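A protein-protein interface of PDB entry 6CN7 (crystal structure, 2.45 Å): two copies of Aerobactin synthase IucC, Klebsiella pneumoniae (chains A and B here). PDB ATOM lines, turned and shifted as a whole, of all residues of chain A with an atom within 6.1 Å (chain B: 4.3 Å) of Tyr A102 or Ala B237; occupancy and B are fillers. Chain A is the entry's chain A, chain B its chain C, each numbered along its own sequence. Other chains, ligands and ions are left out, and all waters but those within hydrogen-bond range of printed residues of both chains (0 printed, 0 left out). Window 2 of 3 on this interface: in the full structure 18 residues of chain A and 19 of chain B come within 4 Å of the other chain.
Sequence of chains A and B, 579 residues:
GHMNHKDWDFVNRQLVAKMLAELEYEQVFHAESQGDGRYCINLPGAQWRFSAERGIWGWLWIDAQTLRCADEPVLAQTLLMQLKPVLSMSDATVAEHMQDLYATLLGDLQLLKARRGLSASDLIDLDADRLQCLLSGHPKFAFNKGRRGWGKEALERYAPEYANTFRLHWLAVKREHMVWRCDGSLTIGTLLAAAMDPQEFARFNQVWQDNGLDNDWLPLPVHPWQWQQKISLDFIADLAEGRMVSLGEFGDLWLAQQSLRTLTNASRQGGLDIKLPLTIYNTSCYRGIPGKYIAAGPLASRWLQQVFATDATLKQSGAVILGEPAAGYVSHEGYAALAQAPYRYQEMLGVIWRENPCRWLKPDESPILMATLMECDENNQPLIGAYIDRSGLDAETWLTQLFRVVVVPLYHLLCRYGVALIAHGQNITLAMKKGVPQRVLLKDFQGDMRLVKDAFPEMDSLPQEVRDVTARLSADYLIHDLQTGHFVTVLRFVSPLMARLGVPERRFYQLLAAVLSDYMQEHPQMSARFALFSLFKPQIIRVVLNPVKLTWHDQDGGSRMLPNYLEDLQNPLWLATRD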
ATOM      1  N   TRP A   8       3.994  20.918 -20.872  1.00  0.00           N
ATOM      2  CA  TRP A   8       3.937  19.545 -21.361  1.00  0.00           C
ATOM      3  C   TRP A   8       4.896  18.644 -20.594  1.00  0.00           C
ATOM      4  O   TRP A   8       4.583  17.480 -20.325  1.00  0.00           O
ATOM      5  CB  TRP A   8       4.245  19.519 -22.859  1.00  0.00           C
ATOM      6  CG  TRP A   8       4.221  18.153 -23.463  1.00  0.00           C
ATOM      7  CD1 TRP A   8       5.286  17.460 -23.957  1.00  0.00           C
ATOM      8  CD2 TRP A   8       3.076  17.311 -23.641  1.00  0.00           C
ATOM      9  NE1 TRP A   8       4.875  16.238 -24.432  1.00  0.00           N
ATOM     10  CE2 TRP A   8       3.522  16.123 -24.251  1.00  0.00           C
ATOM     11  CE3 TRP A   8       1.715  17.447 -23.344  1.00  0.00           C
ATOM     12  CZ2 TRP A   8       2.661  15.075 -24.562  1.00  0.00           C
ATOM     13  CZ3 TRP A   8       0.861  16.407 -23.659  1.00  0.00           C
ATOM     14  CH2 TRP A   8       1.337  15.237 -24.263  1.00  0.00           C
ATOM     15  N   GLN A  77       3.660   8.365 -22.179  1.00  0.00           N
ATOM     16  CA  GLN A  77       3.524   7.438 -23.295  1.00  0.00           C
ATOM     17  C   GLN A  77       4.663   6.424 -23.307  1.00  0.00           C
ATOM     18  O   GLN A  77       4.438   5.227 -23.526  1.00  0.00           O
ATOM     19  CB  GLN A  77       3.478   8.220 -24.607  1.00  0.00           C
ATOM     20  CG  GLN A  77       3.300   7.359 -25.838  1.00  0.00           C
ATOM     21  CD  GLN A  77       4.509   7.376 -26.746  1.00  0.00           C
ATOM     22  OE1 GLN A  77       5.646   7.316 -26.284  1.00  0.00           O
ATOM     23  NE2 GLN A  77       4.270   7.461 -28.051  1.00  0.00           N
ATOM     24  N   HIS A  97      -5.528   2.495 -23.694  1.00  0.00           N
ATOM     25  CA  HIS A  97      -4.921   3.240 -22.598  1.00  0.00           C
ATOM     26  C   HIS A  97      -4.201   4.484 -23.097  1.00  0.00           C
ATOM     27  O   HIS A  97      -4.061   5.457 -22.348  1.00  0.00           O
ATOM     28  CB  HIS A  97      -3.960   2.339 -21.825  1.00  0.00           C
ATOM     29  CG  HIS A  97      -4.650   1.295 -21.001  1.00  0.00           C
ATOM     30  ND1 HIS A  97      -4.070   0.085 -20.691  1.00  0.00           N
ATOM     31  CD2 HIS A  97      -5.873   1.285 -20.420  1.00  0.00           C
ATOM     32  CE1 HIS A  97      -4.905  -0.627 -19.956  1.00  0.00           C
ATOM     33  NE2 HIS A  97      -6.008   0.078 -19.778  1.00  0.00           N
ATOM     34  N   MET A  98      -3.739   4.476 -24.348  1.00  0.00           N
ATOM     35  CA  MET A  98      -3.175   5.687 -24.936  1.00  0.00           C
ATOM     36  C   MET A  98      -4.203   6.806 -24.952  1.00  0.00           C
ATOM     37  O   MET A  98      -3.924   7.931 -24.522  1.00  0.00           O
ATOM     38  CB  MET A  98      -2.679   5.399 -26.352  1.00  0.00           C
ATOM     39  CG  MET A  98      -1.366   4.663 -26.408  1.00  0.00           C
ATOM     40  SD  MET A  98       0.001   5.622 -25.737  1.00  0.00           S
ATOM     41  CE  MET A  98       1.284   4.376 -25.838  1.00  0.00           C
ATOM     42  N   GLN A  99      -5.405   6.516 -25.455  1.00  0.00           N
ATOM     43  CA  GLN A  99      -6.453   7.528 -25.486  1.00  0.00           C
ATOM     44  C   GLN A  99      -6.809   7.988 -24.080  1.00  0.00           C
ATOM     45  O   GLN A  99      -6.945   9.192 -23.830  1.00  0.00           O
ATOM     46  CB  GLN A  99      -7.680   6.981 -26.215  1.00  0.00           C
ATOM     47  CG  GLN A  99      -7.463   6.816 -27.711  1.00  0.00           C
ATOM     48  CD  GLN A  99      -8.657   6.206 -28.416  1.00  0.00           C
ATOM     49  OE1 GLN A  99      -9.551   5.644 -27.781  1.00  0.00           O
ATOM     50  NE2 GLN A  99      -8.681   6.318 -29.740  1.00  0.00           N
ATOM     51  N   ASP A 100      -6.956   7.046 -23.144  1.00  0.00           N
ATOM     52  CA  ASP A 100      -7.155   7.425 -21.749  1.00  0.00           C
ATOM     53  C   ASP A 100      -5.965   8.218 -21.226  1.00  0.00           C
ATOM     54  O   ASP A 100      -6.132   9.171 -20.458  1.00  0.00           O
ATOM     55  CB  ASP A 100      -7.383   6.184 -20.888  1.00  0.00           C
ATOM     56  CG  ASP A 100      -8.668   5.459 -21.236  1.00  0.00           C
ATOM     57  OD1 ASP A 100      -9.574   6.092 -21.817  1.00  0.00           O
ATOM     58  OD2 ASP A 100      -8.774   4.253 -20.923  1.00  0.00           O
ATOM     59  N   LEU A 101      -4.751   7.839 -21.634  1.00  0.00           N
ATOM     60  CA  LEU A 101      -3.559   8.560 -21.201  1.00  0.00           C
ATOM     61  C   LEU A 101      -3.567   9.989 -21.725  1.00  0.00           C
ATOM     62  O   LEU A 101      -3.319  10.939 -20.973  1.00  0.00           O
ATOM     63  CB  LEU A 101      -2.301   7.821 -21.664  1.00  0.00           C
ATOM     64  CG  LEU A 101      -0.939   8.434 -21.314  1.00  0.00           C
ATOM     65  CD1 LEU A 101       0.106   7.335 -21.245  1.00  0.00           C
ATOM     66  CD2 LEU A 101      -0.488   9.497 -22.317  1.00  0.00           C
ATOM     67  N   TYR A 102      -3.838  10.163 -23.019  1.00  0.00           N
ATOM     68  CA  TYR A 102      -3.799  11.499 -23.598  1.00  0.00           C
ATOM     69  C   TYR A 102      -5.003  12.325 -23.170  1.00  0.00           C
ATOM     70  O   TYR A 102      -4.902  13.552 -23.053  1.00  0.00           O
ATOM     71  CB  TYR A 102      -3.707  11.413 -25.122  1.00  0.00           C
ATOM     72  CG  TYR A 102      -2.324  11.034 -25.606  1.00  0.00           C
ATOM     73  CD1 TYR A 102      -1.264  11.921 -25.487  1.00  0.00           C
ATOM     74  CD2 TYR A 102      -2.073   9.789 -26.174  1.00  0.00           C
ATOM     75  CE1 TYR A 102       0.005  11.587 -25.920  1.00  0.00           C
ATOM     76  CE2 TYR A 102      -0.803   9.445 -26.612  1.00  0.00           C
ATOM     77  CZ  TYR A 102       0.230  10.350 -26.481  1.00  0.00           C
ATOM     78  OH  TYR A 102       1.496  10.021 -26.912  1.00  0.00           O
ATOM     79  N   ALA A 103      -6.144  11.680 -22.921  1.00  0.00           N
ATOM     80  CA  ALA A 103      -7.265  12.394 -22.320  1.00  0.00           C
ATOM     81  C   ALA A 103      -6.894  12.950 -20.952  1.00  0.00           C
ATOM     82  O   ALA A 103      -7.354  14.034 -20.574  1.00  0.00           O
ATOM     83  CB  ALA A 103      -8.481  11.476 -22.205  1.00  0.00           C
ATOM     84  N   THR A 104      -6.061  12.227 -20.197  1.00  0.00           N
ATOM     85  CA  THR A 104      -5.647  12.702 -18.880  1.00  0.00           C
ATOM     86  C   THR A 104      -4.676  13.870 -18.998  1.00  0.00           C
ATOM     87  O   THR A 104      -4.793  14.857 -18.260  1.00  0.00           O
ATOM     88  CB  THR A 104      -5.018  11.559 -18.079  1.00  0.00           C
ATOM     89  OG1 THR A 104      -5.968  10.495 -17.934  1.00  0.00           O
ATOM     90  CG2 THR A 104      -4.591  12.036 -16.691  1.00  0.00           C
ATOM     91  N   LEU A 105      -3.710  13.778 -19.914  1.00  0.00           N
ATOM     92  CA  LEU A 105      -2.765  14.874 -20.092  1.00  0.00           C
ATOM     93  C   LEU A 105      -3.471  16.139 -20.560  1.00  0.00           C
ATOM     94  O   LEU A 105      -3.127  17.246 -20.131  1.00  0.00           O
ATOM     95  CB  LEU A 105      -1.675  14.465 -21.083  1.00  0.00           C
ATOM     96  CG  LEU A 105      -0.811  13.269 -20.671  1.00  0.00           C
ATOM     97  CD1 LEU A 105       0.197  12.944 -21.764  1.00  0.00           C
ATOM     98  CD2 LEU A 105      -0.094  13.541 -19.358  1.00  0.00           C
ATOM     99  N   LEU A 106      -4.458  15.998 -21.445  1.00  0.00           N
ATOM    100  CA  LEU A 106      -5.234  17.156 -21.871  1.00  0.00           C
ATOM    101  C   LEU A 106      -5.911  17.820 -20.681  1.00  0.00           C
ATOM    102  O   LEU A 106      -5.856  19.046 -20.525  1.00  0.00           O
ATOM    103  CB  LEU A 106      -6.267  16.737 -22.919  1.00  0.00           C
ATOM    104  CG  LEU A 106      -5.716  16.470 -24.323  1.00  0.00           C
ATOM    105  CD1 LEU A 106      -6.775  15.824 -25.200  1.00  0.00           C
ATOM    106  CD2 LEU A 106      -5.216  17.759 -24.963  1.00  0.00           C
ATOM    107  N   GLY A 107      -6.553  17.023 -19.825  1.00  0.00           N
ATOM    108  CA  GLY A 107      -7.204  17.583 -18.652  1.00  0.00           C
ATOM    109  C   GLY A 107      -6.214  18.186 -17.674  1.00  0.00           C
ATOM    110  O   GLY A 107      -6.463  19.248 -17.099  1.00  0.00           O
ATOM    111  N   LEU A 155     -14.732  15.762 -24.193  1.00  0.00           N
ATOM    112  CA  LEU A 155     -14.068  16.092 -22.936  1.00  0.00           C
ATOM    113  C   LEU A 155     -14.269  17.559 -22.581  1.00  0.00           C
ATOM    114  O   LEU A 155     -14.653  17.894 -21.453  1.00  0.00           O
ATOM    115  CB  LEU A 155     -12.578  15.763 -23.030  1.00  0.00           C
ATOM    116  CG  LEU A 155     -12.217  14.279 -23.167  1.00  0.00           C
ATOM    117  CD1 LEU A 155     -10.763  14.102 -23.589  1.00  0.00           C
ATOM    118  CD2 LEU A 155     -12.481  13.544 -21.862  1.00  0.00           C
ATOM    119  N   PHE B 235      -7.193  10.860 -33.436  1.00  0.00           N
ATOM    120  CA  PHE B 235      -5.956  11.628 -33.479  1.00  0.00           C
ATOM    121  C   PHE B 235      -5.735  12.428 -32.197  1.00  0.00           C
ATOM    122  O   PHE B 235      -5.085  13.476 -32.217  1.00  0.00           O
ATOM    123  CB  PHE B 235      -5.956  12.556 -34.692  1.00  0.00           C
ATOM    124  CG  PHE B 235      -6.034  11.833 -36.006  1.00  0.00           C
ATOM    125  CD1 PHE B 235      -4.895  11.308 -36.592  1.00  0.00           C
ATOM    126  CD2 PHE B 235      -7.243  11.682 -36.655  1.00  0.00           C
ATOM    127  CE1 PHE B 235      -4.966  10.642 -37.800  1.00  0.00           C
ATOM    128  CE2 PHE B 235      -7.321  11.018 -37.864  1.00  0.00           C
ATOM    129  CZ  PHE B 235      -6.182  10.498 -38.438  1.00  0.00           C
ATOM    130  N   ILE B 236      -6.264  11.939 -31.073  1.00  0.00           N
ATOM    131  CA  ILE B 236      -6.150  12.679 -29.821  1.00  0.00           C
ATOM    132  C   ILE B 236      -4.694  12.781 -29.391  1.00  0.00           C
ATOM    133  O   ILE B 236      -4.290  13.773 -28.773  1.00  0.00           O
ATOM    134  CB  ILE B 236      -7.020  12.023 -28.730  1.00  0.00           C
ATOM    135  CG1 ILE B 236      -7.055  12.905 -27.482  1.00  0.00           C
ATOM    136  CG2 ILE B 236      -6.499  10.631 -28.382  1.00  0.00           C
ATOM    137  CD1 ILE B 236      -8.113  12.500 -26.477  1.00  0.00           C
ATOM    138  N   ALA B 237      -3.884  11.769 -29.706  1.00  0.00           N
ATOM    139  CA  ALA B 237      -2.461  11.836 -29.390  1.00  0.00           C
ATOM    140  C   ALA B 237      -1.800  13.007 -30.108  1.00  0.00           C
ATOM    141  O   ALA B 237      -1.038  13.773 -29.505  1.00  0.00           O
ATOM    142  CB  ALA B 237      -1.777  10.521 -29.762  1.00  0.00           C
ATOM    143  N   ASP B 238      -2.087  13.167 -31.402  1.00  0.00           N
ATOM    144  CA  ASP B 238      -1.500  14.269 -32.158  1.00  0.00           C
ATOM    145  C   ASP B 238      -1.962  15.615 -31.616  1.00  0.00           C
ATOM    146  O   ASP B 238      -1.186  16.575 -31.572  1.00  0.00           O
ATOM    147  CB  ASP B 238      -1.855  14.138 -33.640  1.00  0.00           C
ATOM    148  CG  ASP B 238      -1.179  12.952 -34.299  1.00  0.00           C
ATOM    149  OD1 ASP B 238      -0.062  12.588 -33.872  1.00  0.00           O
ATOM    150  OD2 ASP B 238      -1.762  12.385 -35.246  1.00  0.00           O
ATOM    151  N   LEU B 239      -3.227  15.707 -31.199  1.00  0.00           N
ATOM    152  CA  LEU B 239      -3.725  16.951 -30.624  1.00  0.00           C
ATOM    153  C   LEU B 239      -3.093  17.219 -29.264  1.00  0.00           C
ATOM    154  O   LEU B 239      -2.694  18.351 -28.971  1.00  0.00           O
ATOM    155  CB  LEU B 239      -5.247  16.900 -30.505  1.00  0.00           C
ATOM    156  CG  LEU B 239      -6.011  16.748 -31.823  1.00  0.00           C
ATOM    157  CD1 LEU B 239      -7.470  16.415 -31.563  1.00  0.00           C
ATOM    158  CD2 LEU B 239      -5.897  18.013 -32.654  1.00  0.00           C
ATOM    159  N   ALA B 240      -2.987  16.190 -28.420  1.00  0.00           N
ATOM    160  CA  ALA B 240      -2.415  16.378 -27.092  1.00  0.00           C
ATOM    161  C   ALA B 240      -0.957  16.815 -27.171  1.00  0.00           C
ATOM    162  O   ALA B 240      -0.489  17.595 -26.334  1.00  0.00           O
ATOM    163  CB  ALA B 240      -2.542  15.087 -26.281  1.00  0.00           C
ATOM    164  N   GLU B 241      -0.222  16.322 -28.167  1.00  0.00           N
ATOM    165  CA  GLU B 241       1.200  16.612 -28.278  1.00  0.00           C
ATOM    166  C   GLU B 241       1.497  17.888 -29.049  1.00  0.00           C
ATOM    167  O   GLU B 241       2.609  18.413 -28.938  1.00  0.00           O
ATOM    168  CB  GLU B 241       1.922  15.440 -28.949  1.00  0.00           C
ATOM    169  CG  GLU B 241       2.920  14.742 -28.044  1.00  0.00           C
ATOM    170  CD  GLU B 241       3.027  13.253 -28.309  1.00  0.00           C
ATOM    171  OE1 GLU B 241       2.498  12.784 -29.338  1.00  0.00           O
ATOM    172  OE2 GLU B 241       3.636  12.546 -27.475  1.00  0.00           O
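OH of Tyr A102 lies within hydrogen-bond range of OE2 of Glu B241 (3.4 Å).
Ala B240 touches Trp A8 (O to CZ3, 3.2 Å). CZ2 of Trp A8 touches CG of Glu B241, 3.5 Å away. Gln A99 touches Ile B236. Ala B237 touches Tyr A102 (CB to CE2, 3.5 Å). Ala B240 touches Tyr A102 (CB to CD1, 3.5 Å). Leu A106 touches Ile B236. Leu A106 touches Ala B240 (CD2 to CA, 3.8 Å).
Printed residues of chain B within 4 Å of Trp A8: Ala B240 and Glu B241. Of the printed residues of chain B, Gln A99 touches Ile B236 (3.99 Å). Asp A100 touches none of the printed residues of chain B. Thr A104 touches none of the printed residues of chain B. Of the printed residues of chain A, Ile B236 touches Gln A99 and Leu A106. Printed residues of chain A within 4 Å of Glu B241: Trp A8 and Tyr A102. The nearest residue of chain A that does not touch Ala B237 is Trp A8 (5.9 Å). The nearest printed residue of chain B that does not touch Trp A8 is Ala B237 (5.9 Å).
Of the 7 printed residues of chain B, 4 touch a printed residue of chain A. Printed residues of chain B that touch a printed residue of chain A: Ile B236, Ala B237, Ala B240 and Glu B241. Hydrophobic or aromatic side chains of chain B within 4 Å of the printed part of chain A: Ile B236, Ala B237 and Ala B240. Of the 14 printed residues of chain A, 4 touch a printed residue of chain B. Printed residues of chain A that touch a printed residue of chain B: Trp A8, Gln A99, Tyr A102 and Leu A106. Hydrophobic or aromatic side chains of chain A that line the printed part of chain B: Trp A8, Tyr A102 and Leu A106. Among the printed residues, 8 pairs touch across the chains. Among the printed residues, no Asp or Glu carboxylate lies within 4 Å of a Lys or Arg side-chain nitrogen of the other chain.
No position is printed for both chains.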
